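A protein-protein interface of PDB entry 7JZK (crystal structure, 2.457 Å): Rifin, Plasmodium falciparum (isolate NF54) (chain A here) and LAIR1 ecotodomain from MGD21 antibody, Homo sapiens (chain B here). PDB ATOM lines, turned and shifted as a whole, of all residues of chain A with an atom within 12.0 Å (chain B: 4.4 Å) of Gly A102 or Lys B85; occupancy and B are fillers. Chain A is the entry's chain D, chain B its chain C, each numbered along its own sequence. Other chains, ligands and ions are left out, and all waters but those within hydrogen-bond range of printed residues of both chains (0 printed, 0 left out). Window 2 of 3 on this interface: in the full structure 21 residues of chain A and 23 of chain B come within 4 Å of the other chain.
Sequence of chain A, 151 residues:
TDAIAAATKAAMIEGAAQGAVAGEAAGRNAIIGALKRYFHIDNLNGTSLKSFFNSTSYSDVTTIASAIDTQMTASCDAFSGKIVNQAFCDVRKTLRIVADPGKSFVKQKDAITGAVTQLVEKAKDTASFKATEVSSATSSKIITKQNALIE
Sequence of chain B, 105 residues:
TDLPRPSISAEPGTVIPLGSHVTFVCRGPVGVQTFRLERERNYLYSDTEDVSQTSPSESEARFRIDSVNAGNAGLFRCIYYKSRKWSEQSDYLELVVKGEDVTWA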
ATOM      1  N   ARG A  96      -0.555   6.506  -1.973  1.00  0.00           N
ATOM      2  CA  ARG A  96      -1.388   5.679  -2.852  1.00  0.00           C
ATOM      3  C   ARG A  96      -2.853   6.095  -2.759  1.00  0.00           C
ATOM      4  O   ARG A  96      -3.763   5.269  -2.642  1.00  0.00           O
ATOM      5  CB  ARG A  96      -1.202   4.177  -2.590  1.00  0.00           C
ATOM      6  CG  ARG A  96       0.135   3.620  -3.105  1.00  0.00           C
ATOM      7  CD  ARG A  96       0.797   2.703  -2.092  1.00  0.00           C
ATOM      8  NE  ARG A  96       1.246   3.460  -0.926  1.00  0.00           N
ATOM      9  CZ  ARG A  96       1.936   2.946   0.088  1.00  0.00           C
ATOM     10  NH1 ARG A  96       2.299   3.725   1.104  1.00  0.00           N
ATOM     11  NH2 ARG A  96       2.260   1.659   0.084  1.00  0.00           N
ATOM     12  N   ILE A  97      -3.079   7.404  -2.828  1.00  0.00           N
ATOM     13  CA  ILE A  97      -4.434   7.942  -2.801  1.00  0.00           C
ATOM     14  C   ILE A  97      -4.968   8.176  -4.211  1.00  0.00           C
ATOM     15  O   ILE A  97      -6.195   8.259  -4.399  1.00  0.00           O
ATOM     16  CB  ILE A  97      -4.485   9.249  -1.978  1.00  0.00           C
ATOM     17  CG1 ILE A  97      -3.958   9.031  -0.568  1.00  0.00           C
ATOM     18  CG2 ILE A  97      -5.892   9.784  -1.859  1.00  0.00           C
ATOM     19  CD1 ILE A  97      -4.005  10.312   0.241  1.00  0.00           C
ATOM     20  N   VAL A  98      -4.093   8.251  -5.210  1.00  0.00           N
ATOM     21  CA  VAL A  98      -4.561   8.494  -6.562  1.00  0.00           C
ATOM     22  C   VAL A  98      -5.227   7.226  -7.066  1.00  0.00           C
ATOM     23  O   VAL A  98      -4.878   6.111  -6.659  1.00  0.00           O
ATOM     24  CB  VAL A  98      -3.391   8.926  -7.466  1.00  0.00           C
ATOM     25  CG1 VAL A  98      -2.751  10.194  -6.923  1.00  0.00           C
ATOM     26  CG2 VAL A  98      -2.343   7.839  -7.507  1.00  0.00           C
ATOM     27  N   ALA A  99      -6.217   7.391  -7.926  1.00  0.00           N
ATOM     28  CA  ALA A  99      -6.979   6.237  -8.386  1.00  0.00           C
ATOM     29  C   ALA A  99      -6.088   5.356  -9.239  1.00  0.00           C
ATOM     30  O   ALA A  99      -5.373   5.839 -10.118  1.00  0.00           O
ATOM     31  CB  ALA A  99      -8.205   6.683  -9.182  1.00  0.00           C
ATOM     32  N   ASP A 100      -6.122   4.059  -8.993  1.00  0.00           N
ATOM     33  CA  ASP A 100      -5.344   3.129  -9.796  1.00  0.00           C
ATOM     34  C   ASP A 100      -6.358   2.106 -10.306  1.00  0.00           C
ATOM     35  O   ASP A 100      -7.073   1.482  -9.493  1.00  0.00           O
ATOM     36  CB  ASP A 100      -4.197   2.570  -8.935  1.00  0.00           C
ATOM     37  CG  ASP A 100      -3.178   1.742  -9.721  1.00  0.00           C
ATOM     38  OD1 ASP A 100      -3.176   1.736 -10.978  1.00  0.00           O
ATOM     39  OD2 ASP A 100      -2.308   1.144  -9.049  1.00  0.00           O
ATOM     40  N   PRO A 101      -6.546   1.970 -11.617  1.00  0.00           N
ATOM     41  CA  PRO A 101      -7.609   1.074 -12.110  1.00  0.00           C
ATOM     42  C   PRO A 101      -7.418  -0.339 -11.586  1.00  0.00           C
ATOM     43  O   PRO A 101      -6.295  -0.839 -11.476  1.00  0.00           O
ATOM     44  CB  PRO A 101      -7.446   1.128 -13.633  1.00  0.00           C
ATOM     45  CG  PRO A 101      -6.809   2.428 -13.912  1.00  0.00           C
ATOM     46  CD  PRO A 101      -5.962   2.789 -12.691  1.00  0.00           C
ATOM     47  N   GLY A 102      -8.534  -0.968 -11.216  1.00  0.00           N
ATOM     48  CA  GLY A 102      -8.526  -2.351 -10.781  1.00  0.00           C
ATOM     49  C   GLY A 102      -8.351  -2.565  -9.294  1.00  0.00           C
ATOM     50  O   GLY A 102      -8.496  -3.699  -8.827  1.00  0.00           O
ATOM     51  N   LYS A 103      -8.060  -1.523  -8.528  1.00  0.00           N
ATOM     52  CA  LYS A 103      -7.831  -1.681  -7.105  1.00  0.00           C
ATOM     53  C   LYS A 103      -8.888  -0.970  -6.275  1.00  0.00           C
ATOM     54  O   LYS A 103      -9.668  -0.168  -6.767  1.00  0.00           O
ATOM     55  CB  LYS A 103      -6.408  -1.225  -6.760  1.00  0.00           C
ATOM     56  CG  LYS A 103      -5.460  -1.375  -7.952  1.00  0.00           C
ATOM     57  CD  LYS A 103      -4.016  -1.688  -7.567  1.00  0.00           C
ATOM     58  CE  LYS A 103      -3.457  -0.725  -6.532  1.00  0.00           C
ATOM     59  NZ  LYS A 103      -2.142  -1.235  -6.063  1.00  0.00           N
ATOM     60  N   SER A 104      -8.900  -1.318  -4.997  1.00  0.00           N
ATOM     61  CA  SER A 104      -9.880  -0.834  -4.044  1.00  0.00           C
ATOM     62  C   SER A 104      -9.587   0.601  -3.610  1.00  0.00           C
ATOM     63  O   SER A 104      -8.506   1.131  -3.802  1.00  0.00           O
ATOM     64  CB  SER A 104      -9.960  -1.789  -2.842  1.00  0.00           C
ATOM     65  OG  SER A 104      -8.671  -2.248  -2.440  1.00  0.00           O
ATOM     66  N   PHE A 105     -10.612   1.237  -3.065  1.00  0.00           N
ATOM     67  CA  PHE A 105     -10.556   2.632  -2.666  1.00  0.00           C
ATOM     68  C   PHE A 105      -9.608   2.823  -1.491  1.00  0.00           C
ATOM     69  O   PHE A 105      -9.555   1.991  -0.580  1.00  0.00           O
ATOM     70  CB  PHE A 105     -11.952   3.101  -2.279  1.00  0.00           C
ATOM     71  CG  PHE A 105     -12.136   4.578  -2.351  1.00  0.00           C
ATOM     72  CD1 PHE A 105     -12.626   5.154  -3.504  1.00  0.00           C
ATOM     73  CD2 PHE A 105     -11.884   5.388  -1.250  1.00  0.00           C
ATOM     74  CE1 PHE A 105     -12.826   6.501  -3.588  1.00  0.00           C
ATOM     75  CE2 PHE A 105     -12.090   6.752  -1.322  1.00  0.00           C
ATOM     76  CZ  PHE A 105     -12.562   7.317  -2.496  1.00  0.00           C
ATOM     77  N   VAL A 106      -8.838   3.914  -1.518  1.00  0.00           N
ATOM     78  CA  VAL A 106      -8.006   4.323  -0.391  1.00  0.00           C
ATOM     79  C   VAL A 106      -8.470   5.713   0.047  1.00  0.00           C
ATOM     80  O   VAL A 106      -8.345   6.682  -0.711  1.00  0.00           O
ATOM     81  CB  VAL A 106      -6.521   4.304  -0.764  1.00  0.00           C
ATOM     82  CG1 VAL A 106      -5.672   4.724   0.395  1.00  0.00           C
ATOM     83  CG2 VAL A 106      -6.119   2.904  -1.273  1.00  0.00           C
ATOM     84  N   LYS A 107      -9.021   5.821   1.250  1.00  0.00           N
ATOM     85  CA  LYS A 107      -9.497   7.113   1.720  1.00  0.00           C
ATOM     86  C   LYS A 107      -8.349   7.996   2.153  1.00  0.00           C
ATOM     87  O   LYS A 107      -7.437   7.561   2.856  1.00  0.00           O
ATOM     88  CB  LYS A 107     -10.472   6.930   2.875  1.00  0.00           C
ATOM     89  CG  LYS A 107     -11.791   6.373   2.437  1.00  0.00           C
ATOM     90  CD  LYS A 107     -12.435   5.520   3.516  1.00  0.00           C
ATOM     91  CE  LYS A 107     -13.662   4.830   2.954  1.00  0.00           C
ATOM     92  NZ  LYS A 107     -14.825   5.728   3.093  1.00  0.00           N
ATOM     93  N   LEU B   3     -15.269  -3.562 -15.827  1.00  0.00           N
ATOM     94  CA  LEU B   3     -15.877  -2.239 -15.777  1.00  0.00           C
ATOM     95  C   LEU B   3     -15.682  -1.539 -17.115  1.00  0.00           C
ATOM     96  O   LEU B   3     -14.547  -1.426 -17.589  1.00  0.00           O
ATOM     97  CB  LEU B   3     -15.237  -1.402 -14.669  1.00  0.00           C
ATOM     98  CG  LEU B   3     -15.429  -1.862 -13.227  1.00  0.00           C
ATOM     99  CD1 LEU B   3     -14.679  -0.930 -12.232  1.00  0.00           C
ATOM    100  CD2 LEU B   3     -16.928  -1.932 -12.941  1.00  0.00           C
ATOM    101  N   TYR B  80     -14.295   6.147 -12.469  1.00  0.00           N
ATOM    102  CA  TYR B  80     -15.340   5.886 -11.505  1.00  0.00           C
ATOM    103  C   TYR B  80     -14.971   4.665 -10.694  1.00  0.00           C
ATOM    104  O   TYR B  80     -14.115   3.864 -11.083  1.00  0.00           O
ATOM    105  CB  TYR B  80     -16.711   5.712 -12.161  1.00  0.00           C
ATOM    106  CG  TYR B  80     -16.842   4.501 -13.045  1.00  0.00           C
ATOM    107  CD1 TYR B  80     -16.651   4.605 -14.413  1.00  0.00           C
ATOM    108  CD2 TYR B  80     -17.189   3.258 -12.521  1.00  0.00           C
ATOM    109  CE1 TYR B  80     -16.777   3.525 -15.222  1.00  0.00           C
ATOM    110  CE2 TYR B  80     -17.308   2.169 -13.324  1.00  0.00           C
ATOM    111  CZ  TYR B  80     -17.102   2.300 -14.676  1.00  0.00           C
ATOM    112  OH  TYR B  80     -17.231   1.197 -15.501  1.00  0.00           O
ATOM    113  N   TYR B  81     -15.601   4.569  -9.534  1.00  0.00           N
ATOM    114  CA  TYR B  81     -15.367   3.484  -8.597  1.00  0.00           C
ATOM    115  C   TYR B  81     -16.630   2.654  -8.481  1.00  0.00           C
ATOM    116  O   TYR B  81     -17.695   3.190  -8.195  1.00  0.00           O
ATOM    117  CB  TYR B  81     -14.943   4.029  -7.221  1.00  0.00           C
ATOM    118  CG  TYR B  81     -14.412   2.966  -6.263  1.00  0.00           C
ATOM    119  CD1 TYR B  81     -13.113   2.515  -6.344  1.00  0.00           C
ATOM    120  CD2 TYR B  81     -15.219   2.405  -5.277  1.00  0.00           C
ATOM    121  CE1 TYR B  81     -12.636   1.523  -5.478  1.00  0.00           C
ATOM    122  CE2 TYR B  81     -14.735   1.419  -4.411  1.00  0.00           C
ATOM    123  CZ  TYR B  81     -13.452   0.992  -4.516  1.00  0.00           C
ATOM    124  OH  TYR B  81     -12.982   0.042  -3.647  1.00  0.00           O
ATOM    125  N   LYS B  82     -16.516   1.357  -8.724  1.00  0.00           N
ATOM    126  CA  LYS B  82     -17.675   0.477  -8.640  1.00  0.00           C
ATOM    127  C   LYS B  82     -17.225  -0.947  -8.358  1.00  0.00           C
ATOM    128  O   LYS B  82     -16.211  -1.394  -8.888  1.00  0.00           O
ATOM    129  CB  LYS B  82     -18.474   0.634  -9.943  1.00  0.00           C
ATOM    130  CG  LYS B  82     -19.920   0.213  -9.977  1.00  0.00           C
ATOM    131  CD  LYS B  82     -20.191  -1.133 -10.617  1.00  0.00           C
ATOM    132  CE  LYS B  82     -21.339  -0.921 -11.615  1.00  0.00           C
ATOM    133  NZ  LYS B  82     -21.553  -1.963 -12.659  1.00  0.00           N
ATOM    134  N   SER B  83     -17.969  -1.631  -7.491  1.00  0.00           N
ATOM    135  CA  SER B  83     -17.674  -3.007  -7.097  1.00  0.00           C
ATOM    136  C   SER B  83     -16.223  -3.168  -6.626  1.00  0.00           C
ATOM    137  O   SER B  83     -15.477  -4.023  -7.100  1.00  0.00           O
ATOM    138  CB  SER B  83     -18.010  -3.965  -8.241  1.00  0.00           C
ATOM    139  OG  SER B  83     -19.185  -3.543  -8.922  1.00  0.00           O
ATOM    140  N   ARG B  84     -15.801  -2.301  -5.703  1.00  0.00           N
ATOM    141  CA  ARG B  84     -14.476  -2.388  -5.063  1.00  0.00           C
ATOM    142  C   ARG B  84     -13.306  -2.227  -6.016  1.00  0.00           C
ATOM    143  O   ARG B  84     -12.242  -2.785  -5.783  1.00  0.00           O
ATOM    144  CB  ARG B  84     -14.286  -3.683  -4.295  1.00  0.00           C
ATOM    145  CG  ARG B  84     -15.361  -4.010  -3.314  1.00  0.00           C
ATOM    146  CD  ARG B  84     -15.512  -5.518  -3.290  1.00  0.00           C
ATOM    147  NE  ARG B  84     -16.910  -5.899  -3.360  1.00  0.00           N
ATOM    148  CZ  ARG B  84     -17.350  -7.015  -3.920  1.00  0.00           C
ATOM    149  NH1 ARG B  84     -18.646  -7.272  -3.936  1.00  0.00           N
ATOM    150  NH2 ARG B  84     -16.497  -7.861  -4.471  1.00  0.00           N
ATOM    151  N   LYS B  85     -13.491  -1.537  -7.128  1.00  0.00           N
ATOM    152  CA  LYS B  85     -12.354  -1.298  -7.993  1.00  0.00           C
ATOM    153  C   LYS B  85     -12.562  -0.023  -8.763  1.00  0.00           C
ATOM    154  O   LYS B  85     -13.677   0.317  -9.133  1.00  0.00           O
ATOM    155  CB  LYS B  85     -12.059  -2.468  -8.949  1.00  0.00           C
ATOM    156  CG  LYS B  85     -13.221  -3.077  -9.660  1.00  0.00           C
ATOM    157  CD  LYS B  85     -12.810  -4.480 -10.125  1.00  0.00           C
ATOM    158  CE  LYS B  85     -12.190  -5.276  -8.986  1.00  0.00           C
ATOM    159  NZ  LYS B  85     -12.037  -6.721  -9.315  1.00  0.00           N
ATOM    160  N   TRP B  86     -11.472   0.688  -8.965  1.00  0.00           N
ATOM    161  CA  TRP B  86     -11.500   1.818  -9.866  1.00  0.00           C
ATOM    162  C   TRP B  86     -11.580   1.268 -11.280  1.00  0.00           C
ATOM    163  O   TRP B  86     -10.942   0.265 -11.600  1.00  0.00           O
ATOM    164  CB  TRP B  86     -10.229   2.661  -9.711  1.00  0.00           C
ATOM    165  CG  TRP B  86     -10.225   3.557  -8.537  1.00  0.00           C
ATOM    166  CD1 TRP B  86      -9.447   3.440  -7.418  1.00  0.00           C
ATOM    167  CD2 TRP B  86     -10.994   4.747  -8.371  1.00  0.00           C
ATOM    168  NE1 TRP B  86      -9.710   4.471  -6.552  1.00  0.00           N
ATOM    169  CE2 TRP B  86     -10.652   5.293  -7.117  1.00  0.00           C
ATOM    170  CE3 TRP B  86     -11.944   5.401  -9.157  1.00  0.00           C
ATOM    171  CZ2 TRP B  86     -11.233   6.461  -6.628  1.00  0.00           C
ATOM    172  CZ3 TRP B  86     -12.523   6.560  -8.670  1.00  0.00           C
ATOM    173  CH2 TRP B  86     -12.164   7.077  -7.420  1.00  0.00           C
ATOM    174  N   SER B  87     -12.349   1.929 -12.127  1.00  0.00           N
ATOM    175  CA  SER B  87     -12.346   1.619 -13.541  1.00  0.00           C
ATOM    176  C   SER B  87     -11.102   2.199 -14.209  1.00  0.00           C
ATOM    177  O   SER B  87     -10.341   2.962 -13.606  1.00  0.00           O
ATOM    178  CB  SER B  87     -13.578   2.200 -14.187  1.00  0.00           C
ATOM    179  OG  SER B  87     -13.443   3.588 -14.176  1.00  0.00           O
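The side-chain hydroxyl of Tyr B81 is in hydrogen-bond range of the backbone NH of Phe A105, at 2.7 Å.
The backbone carbonyl oxygen of Trp B86 is in hydrogen-bond range of the backbone NH of Gly A102 (2.7 Å).
N of Trp B86 lies within hydrogen-bond range of O of Lys A103 (3.0 Å).
The backbone carbonyl oxygen of Tyr B80 is in hydrogen-bond range of the backbone NH of Ser B87, at 2.8 Å.
OD2 of Asp A100 is in salt-bridge range of NZ of Lys A103 (3.8 Å).
Ala A99 touches Trp B86.
CB of Trp B86 touches O of Asp A100, at 3.4 Å.
O of Trp B86 touches CA of Pro A101, at 3.5 Å.
CB of Pro A101 touches O of Ser B87 (3.4 Å).
Gly A102 touches Lys B85.
O of Lys A103 touches CE1 of Tyr B81, 3.7 Å away.
Arg B84 touches Lys A103.
Ser A104 touches Tyr B81 (CA to OH, 3.2 Å).
CA of Ser A104 touches O of Arg B84, at 3.5 Å.
Trp B86 touches Phe A105 (CZ2 to CE1, 3.4 Å).
Gly A102 touches just these residues of chain B: Lys B85 and Trp B86.
Lys B85 touches two residues of chain A.
Tyr B81 touches just these residues of chain A: Lys A103, Ser A104 and Phe A105.
Of chain A, only Ala A99 (3.5 Å), Asp A100 (3.4 Å), Pro A101 (3.5 Å), Gly A102 (2.7 Å), Lys A103 (3.0 Å) and Phe A105 (3.4 Å) come within 4 Å of Trp B86.
Printed residues of chain B within 4 Å of Phe A105: Tyr B81 and Trp B86.
Printed residues of chain B within 4 Å of Ser A104: Tyr B81 (3.2 Å) and Arg B84 (3.5 Å).
Printed residues of chain B within 4 Å of Pro A101: Trp B86 and Ser B87.
Of the printed residues of chain B, Asp A100 touches Trp B86.
Printed residues of chain B within 4 Å of Ala A99: Trp B86.
Lys A107 touches none of the printed residues of chain B.
The nearest printed residue of chain B that does not touch Gly A102 is Ser B87 (4.9 Å).
The nearest residue of chain A that does not touch Lys B85 is Ser A104 (4.6 Å).
The nearest printed residue of chain B that does not touch Ala A99 is Ser B87 (6.2 Å).
Of the 9 printed residues of chain B, 5 touch a printed residue of chain A.
Hydrophobic or aromatic side chains of chain B within 4 Å of the printed part of chain A: Tyr B81 and Trp B86.
Of the 12 printed residues of chain A, 7 touch a printed residue of chain B.
Printed residues of chain A that touch a printed residue of chain B: Ala A99, Asp A100, Pro A101, Gly A102, Lys A103, Ser A104 and Phe A105.
Hydrophobic or aromatic side chains of chain A that line the printed part of chain B: Ala A99, Pro A101 and Phe A105.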
